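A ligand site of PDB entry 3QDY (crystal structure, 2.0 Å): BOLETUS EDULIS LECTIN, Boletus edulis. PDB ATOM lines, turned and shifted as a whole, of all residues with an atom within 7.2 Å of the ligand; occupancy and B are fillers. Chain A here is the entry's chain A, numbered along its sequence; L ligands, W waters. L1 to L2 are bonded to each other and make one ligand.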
ATOM      1  N   PHE A  27      15.205 -19.095 -13.037  1.00  0.00           N
ATOM      2  CA  PHE A  27      14.021 -19.925 -12.827  1.00  0.00           C
ATOM      3  C   PHE A  27      13.825 -20.194 -11.337  1.00  0.00           C
ATOM      4  O   PHE A  27      14.782 -20.158 -10.559  1.00  0.00           O
ATOM      5  CB  PHE A  27      14.127 -21.226 -13.622  1.00  0.00           C
ATOM      6  CG  PHE A  27      12.802 -21.934 -13.811  1.00  0.00           C
ATOM      7  CD1 PHE A  27      12.537 -23.121 -13.153  1.00  0.00           C
ATOM      8  CD2 PHE A  27      11.825 -21.390 -14.632  1.00  0.00           C
ATOM      9  CE1 PHE A  27      11.316 -23.769 -13.326  1.00  0.00           C
ATOM     10  CE2 PHE A  27      10.601 -22.024 -14.808  1.00  0.00           C
ATOM     11  CZ  PHE A  27      10.341 -23.218 -14.154  1.00  0.00           C
ATOM     12  N   HIS A  28      12.588 -20.459 -10.947  1.00  0.00           N
ATOM     13  CA  HIS A  28      12.206 -20.448  -9.536  1.00  0.00           C
ATOM     14  C   HIS A  28      12.444 -21.764  -8.783  1.00  0.00           C
ATOM     15  O   HIS A  28      12.234 -21.824  -7.570  1.00  0.00           O
ATOM     16  CB  HIS A  28      10.749 -19.993  -9.365  1.00  0.00           C
ATOM     17  CG  HIS A  28       9.748 -20.928  -9.969  1.00  0.00           C
ATOM     18  ND1 HIS A  28       9.306 -20.815 -11.269  1.00  0.00           N
ATOM     19  CD2 HIS A  28       9.099 -21.995  -9.435  1.00  0.00           C
ATOM     20  CE1 HIS A  28       8.423 -21.775 -11.514  1.00  0.00           C
ATOM     21  NE2 HIS A  28       8.284 -22.508 -10.425  1.00  0.00           N
ATOM     22  N   TYR A  29      12.870 -22.803  -9.492  1.00  0.00           N
ATOM     23  CA  TYR A  29      13.169 -24.078  -8.842  1.00  0.00           C
ATOM     24  C   TYR A  29      14.419 -23.980  -7.980  1.00  0.00           C
ATOM     25  O   TYR A  29      15.157 -22.996  -8.053  1.00  0.00           O
ATOM     26  CB  TYR A  29      13.359 -25.202  -9.877  1.00  0.00           C
ATOM     27  CG  TYR A  29      12.080 -25.719 -10.491  1.00  0.00           C
ATOM     28  CD1 TYR A  29      12.116 -26.575 -11.589  1.00  0.00           C
ATOM     29  CD2 TYR A  29      10.841 -25.353  -9.985  1.00  0.00           C
ATOM     30  CE1 TYR A  29      10.958 -27.058 -12.160  1.00  0.00           C
ATOM     31  CE2 TYR A  29       9.671 -25.826 -10.540  1.00  0.00           C
ATOM     32  CZ  TYR A  29       9.736 -26.681 -11.628  1.00  0.00           C
ATOM     33  OH  TYR A  29       8.573 -27.156 -12.195  1.00  0.00           O
ATOM     34  N   ALA A  30      14.636 -25.004  -7.162  1.00  0.00           N
ATOM     35  CA  ALA A  30      15.867 -25.122  -6.362  1.00  0.00           C
ATOM     36  C   ALA A  30      16.179 -23.886  -5.532  1.00  0.00           C
ATOM     37  O   ALA A  30      17.351 -23.569  -5.286  1.00  0.00           O
ATOM     38  CB  ALA A  30      17.053 -25.497  -7.255  1.00  0.00           C
ATOM     39  N   ASN A  31      15.138 -23.179  -5.105  1.00  0.00           N
ATOM     40  CA  ASN A  31      15.302 -22.015  -4.251  1.00  0.00           C
ATOM     41  C   ASN A  31      15.826 -20.807  -5.023  1.00  0.00           C
ATOM     42  O   ASN A  31      16.472 -19.922  -4.451  1.00  0.00           O
ATOM     43  CB  ASN A  31      16.235 -22.347  -3.083  1.00  0.00           C
ATOM     44  CG  ASN A  31      15.668 -21.909  -1.757  1.00  0.00           C
ATOM     45  OD1 ASN A  31      14.491 -22.152  -1.459  1.00  0.00           O
ATOM     46  ND2 ASN A  31      16.492 -21.264  -0.938  1.00  0.00           N
ATOM     47  N   GLY A  32      15.545 -20.770  -6.322  1.00  0.00           N
ATOM     48  CA  GLY A  32      15.935 -19.634  -7.154  1.00  0.00           C
ATOM     49  C   GLY A  32      17.427 -19.469  -7.321  1.00  0.00           C
ATOM     50  O   GLY A  32      18.181 -20.444  -7.285  1.00  0.00           O
ATOM     51  N   GLY A  48      20.591 -24.713  -5.403  1.00  0.00           N
ATOM     52  CA  GLY A  48      20.784 -26.159  -5.460  1.00  0.00           C
ATOM     53  C   GLY A  48      20.661 -26.672  -6.878  1.00  0.00           C
ATOM     54  O   GLY A  48      20.504 -25.887  -7.814  1.00  0.00           O
ATOM     55  N   SER A  49      20.731 -27.986  -7.049  1.00  0.00           N
ATOM     56  CA  SER A  49      20.541 -28.580  -8.369  1.00  0.00           C
ATOM     57  C   SER A  49      19.067 -28.540  -8.769  1.00  0.00           C
ATOM     58  O   SER A  49      18.186 -28.754  -7.932  1.00  0.00           O
ATOM     59  CB  SER A  49      21.039 -30.026  -8.383  1.00  0.00           C
ATOM     60  OG  SER A  49      20.825 -30.634  -9.658  1.00  0.00           O
ATOM     61  N   GLY A  50      18.800 -28.245 -10.041  1.00  0.00           N
ATOM     62  CA  GLY A  50      17.437 -28.322 -10.552  1.00  0.00           C
ATOM     63  C   GLY A  50      16.856 -27.019 -11.060  1.00  0.00           C
ATOM     64  O   GLY A  50      15.665 -26.944 -11.361  1.00  0.00           O
ATOM     65  N   THR A  51      17.678 -25.977 -11.164  1.00  0.00           N
ATOM     66  CA  THR A  51      17.205 -24.730 -11.753  1.00  0.00           C
ATOM     67  C   THR A  51      18.188 -24.195 -12.782  1.00  0.00           C
ATOM     68  O   THR A  51      19.162 -24.860 -13.124  1.00  0.00           O
ATOM     69  CB  THR A  51      16.864 -23.660 -10.682  1.00  0.00           C
ATOM     70  OG1 THR A  51      16.111 -22.609 -11.282  1.00  0.00           O
ATOM     71  CG2 THR A  51      18.137 -23.094 -10.047  1.00  0.00           C
ATOM     72  N   VAL A  71      21.817 -26.459 -13.861  1.00  0.00           N
ATOM     73  CA  VAL A  71      22.259 -27.745 -13.338  1.00  0.00           C
ATOM     74  C   VAL A  71      21.052 -28.663 -13.239  1.00  0.00           C
ATOM     75  O   VAL A  71      20.055 -28.344 -12.580  1.00  0.00           O
ATOM     76  CB  VAL A  71      22.922 -27.599 -11.949  1.00  0.00           C
ATOM     77  CG1 VAL A  71      23.341 -28.969 -11.418  1.00  0.00           C
ATOM     78  CG2 VAL A  71      24.137 -26.673 -12.025  1.00  0.00           C
ATOM     79  N   HIS A  72      21.134 -29.811 -13.904  1.00  0.00           N
ATOM     80  CA  HIS A  72      20.051 -30.771 -13.922  1.00  0.00           C
ATOM     81  C   HIS A  72      20.511 -32.122 -13.350  1.00  0.00           C
ATOM     82  O   HIS A  72      21.354 -32.790 -13.935  1.00  0.00           O
ATOM     83  CB  HIS A  72      19.520 -30.955 -15.345  1.00  0.00           C
ATOM     84  CG  HIS A  72      18.455 -32.013 -15.455  1.00  0.00           C
ATOM     85  ND1 HIS A  72      18.656 -33.175 -16.166  1.00  0.00           N
ATOM     86  CD2 HIS A  72      17.207 -32.087 -14.941  1.00  0.00           C
ATOM     87  CE1 HIS A  72      17.563 -33.930 -16.088  1.00  0.00           C
ATOM     88  NE2 HIS A  72      16.670 -33.279 -15.352  1.00  0.00           N
ATOM     89  N   ASN A  73      19.956 -32.485 -12.199  1.00  0.00           N
ATOM     90  CA  ASN A  73      20.353 -33.711 -11.517  1.00  0.00           C
ATOM     91  C   ASN A  73      21.854 -33.775 -11.268  1.00  0.00           C
ATOM     92  O   ASN A  73      22.481 -34.820 -11.444  1.00  0.00           O
ATOM     93  CB  ASN A  73      19.859 -34.950 -12.271  1.00  0.00           C
ATOM     94  CG  ASN A  73      18.361 -35.175 -12.099  1.00  0.00           C
ATOM     95  OD1 ASN A  73      17.785 -34.810 -11.076  1.00  0.00           O
ATOM     96  ND2 ASN A  73      17.733 -35.778 -13.103  1.00  0.00           N
ATOM     97  N   TYR A  74      22.424 -32.642 -10.876  1.00  0.00           N
ATOM     98  CA  TYR A  74      23.821 -32.572 -10.435  1.00  0.00           C
ATOM     99  C   TYR A  74      24.834 -32.506 -11.580  1.00  0.00           C
ATOM    100  O   TYR A  74      26.041 -32.551 -11.343  1.00  0.00           O
ATOM    101  CB  TYR A  74      24.130 -33.725  -9.472  1.00  0.00           C
ATOM    102  CG  TYR A  74      23.072 -33.874  -8.404  1.00  0.00           C
ATOM    103  CD1 TYR A  74      22.163 -34.919  -8.437  1.00  0.00           C
ATOM    104  CD2 TYR A  74      22.965 -32.939  -7.376  1.00  0.00           C
ATOM    105  CE1 TYR A  74      21.187 -35.053  -7.471  1.00  0.00           C
ATOM    106  CE2 TYR A  74      21.992 -33.063  -6.402  1.00  0.00           C
ATOM    107  CZ  TYR A  74      21.109 -34.122  -6.449  1.00  0.00           C
ATOM    108  OH  TYR A  74      20.144 -34.247  -5.486  1.00  0.00           O
ATOM    109  N   LYS A  75      24.336 -32.379 -12.799  1.00  0.00           N
ATOM    110  CA  LYS A  75      25.210 -32.220 -13.951  1.00  0.00           C
ATOM    111  C   LYS A  75      24.861 -30.934 -14.687  1.00  0.00           C
ATOM    112  O   LYS A  75      23.679 -30.581 -14.804  1.00  0.00           O
ATOM    113  CB  LYS A  75      25.067 -33.410 -14.906  1.00  0.00           C
ATOM    114  CG  LYS A  75      25.576 -34.734 -14.348  1.00  0.00           C
ATOM    115  CD  LYS A  75      25.381 -35.852 -15.360  1.00  0.00           C
ATOM    116  CE  LYS A  75      25.884 -37.178 -14.831  1.00  0.00           C
ATOM    117  NZ  LYS A  75      25.583 -38.281 -15.779  1.00  0.00           N
ATOM    118  N   TYR A  97      11.997 -24.508 -20.624  1.00  0.00           N
ATOM    119  CA  TYR A  97      12.868 -25.646 -20.344  1.00  0.00           C
ATOM    120  C   TYR A  97      12.252 -26.577 -19.285  1.00  0.00           C
ATOM    121  O   TYR A  97      12.827 -27.602 -18.948  1.00  0.00           O
ATOM    122  CB  TYR A  97      14.256 -25.180 -19.898  1.00  0.00           C
ATOM    123  CG  TYR A  97      15.056 -24.520 -21.003  1.00  0.00           C
ATOM    124  CD1 TYR A  97      15.032 -23.143 -21.182  1.00  0.00           C
ATOM    125  CD2 TYR A  97      15.838 -25.282 -21.872  1.00  0.00           C
ATOM    126  CE1 TYR A  97      15.750 -22.546 -22.194  1.00  0.00           C
ATOM    127  CE2 TYR A  97      16.558 -24.679 -22.891  1.00  0.00           C
ATOM    128  CZ  TYR A  97      16.515 -23.303 -23.040  1.00  0.00           C
ATOM    129  OH  TYR A  97      17.227 -22.698 -24.048  1.00  0.00           O
ATOM    130  N   TYR A  98      11.094 -26.192 -18.762  1.00  0.00           N
ATOM    131  CA  TYR A  98      10.473 -26.950 -17.693  1.00  0.00           C
ATOM    132  C   TYR A  98       8.994 -27.248 -17.969  1.00  0.00           C
ATOM    133  O   TYR A  98       8.433 -26.783 -18.961  1.00  0.00           O
ATOM    134  CB  TYR A  98      10.637 -26.212 -16.353  1.00  0.00           C
ATOM    135  CG  TYR A  98      12.076 -25.943 -15.996  1.00  0.00           C
ATOM    136  CD1 TYR A  98      12.732 -24.817 -16.457  1.00  0.00           C
ATOM    137  CD2 TYR A  98      12.787 -26.834 -15.201  1.00  0.00           C
ATOM    138  CE1 TYR A  98      14.060 -24.572 -16.144  1.00  0.00           C
ATOM    139  CE2 TYR A  98      14.118 -26.597 -14.868  1.00  0.00           C
ATOM    140  CZ  TYR A  98      14.747 -25.467 -15.348  1.00  0.00           C
ATOM    141  OH  TYR A  98      16.070 -25.234 -15.020  1.00  0.00           O
ATOM    142  N   ASN A  99       8.375 -28.024 -17.093  1.00  0.00           N
ATOM    143  CA  ASN A  99       6.957 -28.353 -17.229  1.00  0.00           C
ATOM    144  C   ASN A  99       6.628 -28.887 -18.619  1.00  0.00           C
ATOM    145  O   ASN A  99       5.612 -28.523 -19.212  1.00  0.00           O
ATOM    146  CB  ASN A  99       6.106 -27.122 -16.917  1.00  0.00           C
ATOM    147  CG  ASN A  99       6.284 -26.642 -15.491  1.00  0.00           C
ATOM    148  OD1 ASN A  99       6.001 -27.364 -14.535  1.00  0.00           O
ATOM    149  ND2 ASN A  99       6.755 -25.401 -15.338  1.00  0.00           N
ATOM    150  N   ASN A 100       7.510 -29.746 -19.137  1.00  0.00           N
ATOM    151  CA  ASN A 100       7.317 -30.346 -20.450  1.00  0.00           C
ATOM    152  C   ASN A 100       7.233 -29.317 -21.567  1.00  0.00           C
ATOM    153  O   ASN A 100       6.593 -29.540 -22.591  1.00  0.00           O
ATOM    154  CB  ASN A 100       6.065 -31.228 -20.457  1.00  0.00           C
ATOM    155  CG  ASN A 100       6.177 -32.408 -19.519  1.00  0.00           C
ATOM    156  OD1 ASN A 100       7.133 -33.184 -19.588  1.00  0.00           O
ATOM    157  ND2 ASN A 100       5.194 -32.559 -18.633  1.00  0.00           N
ATOM    158  N   ALA A 104      12.679 -28.433 -22.871  1.00  0.00           N
ATOM    159  CA  ALA A 104      13.070 -29.329 -21.793  1.00  0.00           C
ATOM    160  C   ALA A 104      14.018 -30.434 -22.276  1.00  0.00           C
ATOM    161  O   ALA A 104      14.846 -30.923 -21.505  1.00  0.00           O
ATOM    162  CB  ALA A 104      11.838 -29.933 -21.136  1.00  0.00           C
ATOM    163  N   ARG A 107      17.687 -29.413 -22.089  1.00  0.00           N
ATOM    164  CA  ARG A 107      18.125 -29.433 -20.696  1.00  0.00           C
ATOM    165  C   ARG A 107      18.448 -30.847 -20.205  1.00  0.00           C
ATOM    166  O   ARG A 107      19.393 -31.057 -19.445  1.00  0.00           O
ATOM    167  CB  ARG A 107      17.065 -28.823 -19.765  1.00  0.00           C
ATOM    168  CG  ARG A 107      17.254 -29.202 -18.299  1.00  0.00           C
ATOM    169  CD  ARG A 107      16.205 -28.584 -17.371  1.00  0.00           C
ATOM    170  NE  ARG A 107      14.835 -28.919 -17.740  1.00  0.00           N
ATOM    171  CZ  ARG A 107      14.209 -30.049 -17.387  1.00  0.00           C
ATOM    172  NH1 ARG A 107      14.831 -30.953 -16.659  1.00  0.00           N
ATOM    173  NH2 ARG A 107      12.962 -30.255 -17.772  1.00  0.00           N
ATOM    174  N   GLU A 108      17.639 -31.814 -20.623  1.00  0.00           N
ATOM    175  CA  GLU A 108      17.789 -33.194 -20.169  1.00  0.00           C
ATOM    176  C   GLU A 108      19.076 -33.846 -20.688  1.00  0.00           C
ATOM    177  O   GLU A 108      19.559 -34.819 -20.112  1.00  0.00           O
ATOM    178  CB  GLU A 108      16.553 -34.013 -20.538  1.00  0.00           C
ATOM    179  CG  GLU A 108      15.318 -33.627 -19.731  1.00  0.00           C
ATOM    180  CD  GLU A 108      14.013 -34.110 -20.342  1.00  0.00           C
ATOM    181  OE1 GLU A 108      14.006 -34.478 -21.534  1.00  0.00           O
ATOM    182  OE2 GLU A 108      12.994 -34.107 -19.626  1.00  0.00           O
HETATM  183  O1  LIG L   1      14.443 -31.898 -12.971  1.00  0.00           O
HETATM  184  C1  LIG L   1      15.170 -32.532 -11.891  1.00  0.00           C
HETATM  185  O2  LIG L   1      14.351 -33.559 -11.323  1.00  0.00           O
HETATM  186  C2  LIG L   1      15.547 -31.515 -10.800  1.00  0.00           C
HETATM  187  N1  LIG L   1      16.174 -32.204  -9.666  1.00  0.00           N
HETATM  188  C3  LIG L   1      14.298 -30.782 -10.310  1.00  0.00           C
HETATM  189  O3  LIG L   1      14.672 -29.738  -9.407  1.00  0.00           O
HETATM  190  C4  LIG L   1      13.548 -30.199 -11.501  1.00  0.00           C
HETATM  191  O4  LIG L   1      14.359 -29.208 -12.137  1.00  0.00           O
HETATM  192  C5  LIG L   1      13.220 -31.308 -12.501  1.00  0.00           C
HETATM  193  C6  LIG L   1      12.426 -30.694 -13.658  1.00  0.00           C
HETATM  194  O5  LIG L   1      12.151 -31.693 -14.649  1.00  0.00           O
HETATM  195  C7  LIG L   1      17.473 -32.097  -9.426  1.00  0.00           C
HETATM  196  O6  LIG L   1      18.251 -31.469 -10.136  1.00  0.00           O
HETATM  197  C8  LIG L   1      17.979 -32.867  -8.188  1.00  0.00           C
HETATM  198  C1  LG2 L   2      13.789 -29.616  -8.284  1.00  0.00           C
HETATM  199  C2  LG2 L   2      14.491 -28.754  -7.231  1.00  0.00           C
HETATM  200  C3  LG2 L   2      13.608 -28.608  -6.000  1.00  0.00           C
HETATM  201  C4  LG2 L   2      12.236 -28.099  -6.417  1.00  0.00           C
HETATM  202  C5  LG2 L   2      11.645 -28.993  -7.493  1.00  0.00           C
HETATM  203  C6  LG2 L   2      10.285 -28.461  -7.942  1.00  0.00           C
HETATM  204  O1  LG2 L   2      15.737 -29.336  -6.886  1.00  0.00           O
HETATM  205  O2  LG2 L   2      14.183 -27.710  -5.082  1.00  0.00           O
HETATM  206  O3  LG2 L   2      12.362 -26.782  -6.925  1.00  0.00           O
HETATM  207  O4  LG2 L   2      12.532 -29.057  -8.598  1.00  0.00           O
HETATM  208  O5  LG2 L   2       9.631 -29.420  -8.738  1.00  0.00           O
HETATM  209  O   HOH W   1      16.555 -29.494 -13.785  1.00  0.00           O
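OG of Ser 49 sits at hydrogen-bond distance from O6 of LIG L1 (2.7 Å).
O4 of LIG L1 sits at hydrogen-bond distance from O of Gly 50 (2.7 Å).
N of Ala 30 is in hydrogen-bond range of O3 of LG2 L2 (2.9 Å).
OD1 of Asn 73 sits close to N1 of LIG L1 (3.4 Å).
O of Ser 49 lies within hydrogen-bond range of O1 of LG2 L2, at 2.7 Å.
NH1 of Arg 107 lies within hydrogen-bond range of O5 of LIG L1 (3.4 Å).
The backbone NH of Asn 73 is in hydrogen-bond range of an oxygen (O6) of LIG L1, 2.9 Å away.
An oxygen (O6) of LIG L1 lies within hydrogen-bond range of the backbone NH of Gly 50, at 3.3 Å.
CA of Tyr 29 touches O3 of LG2 L2 (3.4 Å).
CD2 of His 72 touches O1 of LIG L1, at 3.4 Å.
OH of Tyr 74 touches C8 of LIG L1, 3.7 Å away.
CE2 of Tyr 98 touches O4 of LIG L1, at 3.8 Å.
Hydrophobic or aromatic side chains within 4 Å of the ligand: Tyr 29, His 72, Tyr 74 and Tyr 98.
Of the 22 residues printed, 9 come within 4 Å of the ligand.
The nearest printed residue that does not touch the ligand is Val 71 (4.4 Å).
The backbone NH (N) of Tyr 74 sits at hydrogen-bond distance from the side-chain hydroxyl (OG) of Ser 49 (2.8 Å).
NE of Arg 107 sits at hydrogen-bond distance from O of Tyr 97 (2.7 Å).
A ring nitrogen (NE2) of His 72 lies close to the guanidinium group (NH1) of Arg 107.
The side-chain hydroxyl (OG1) of Thr 51 lies close to the backbone carbonyl oxygen (O) of Tyr 29 (3.4 Å).
The backbone carbonyl oxygen of Ala 30 sits at hydrogen-bond distance from the backbone NH of Gly 48, 3.4 Å away.
OH of Tyr 29 lies within hydrogen-bond range of OD1 of Asn 99, at 3.5 Å.
OG of Ser 49 sits at hydrogen-bond distance from N of Asn 73, at 3.3 Å.
N of Gly 50 is in hydrogen-bond range of O of Val 71, 2.8 Å away.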
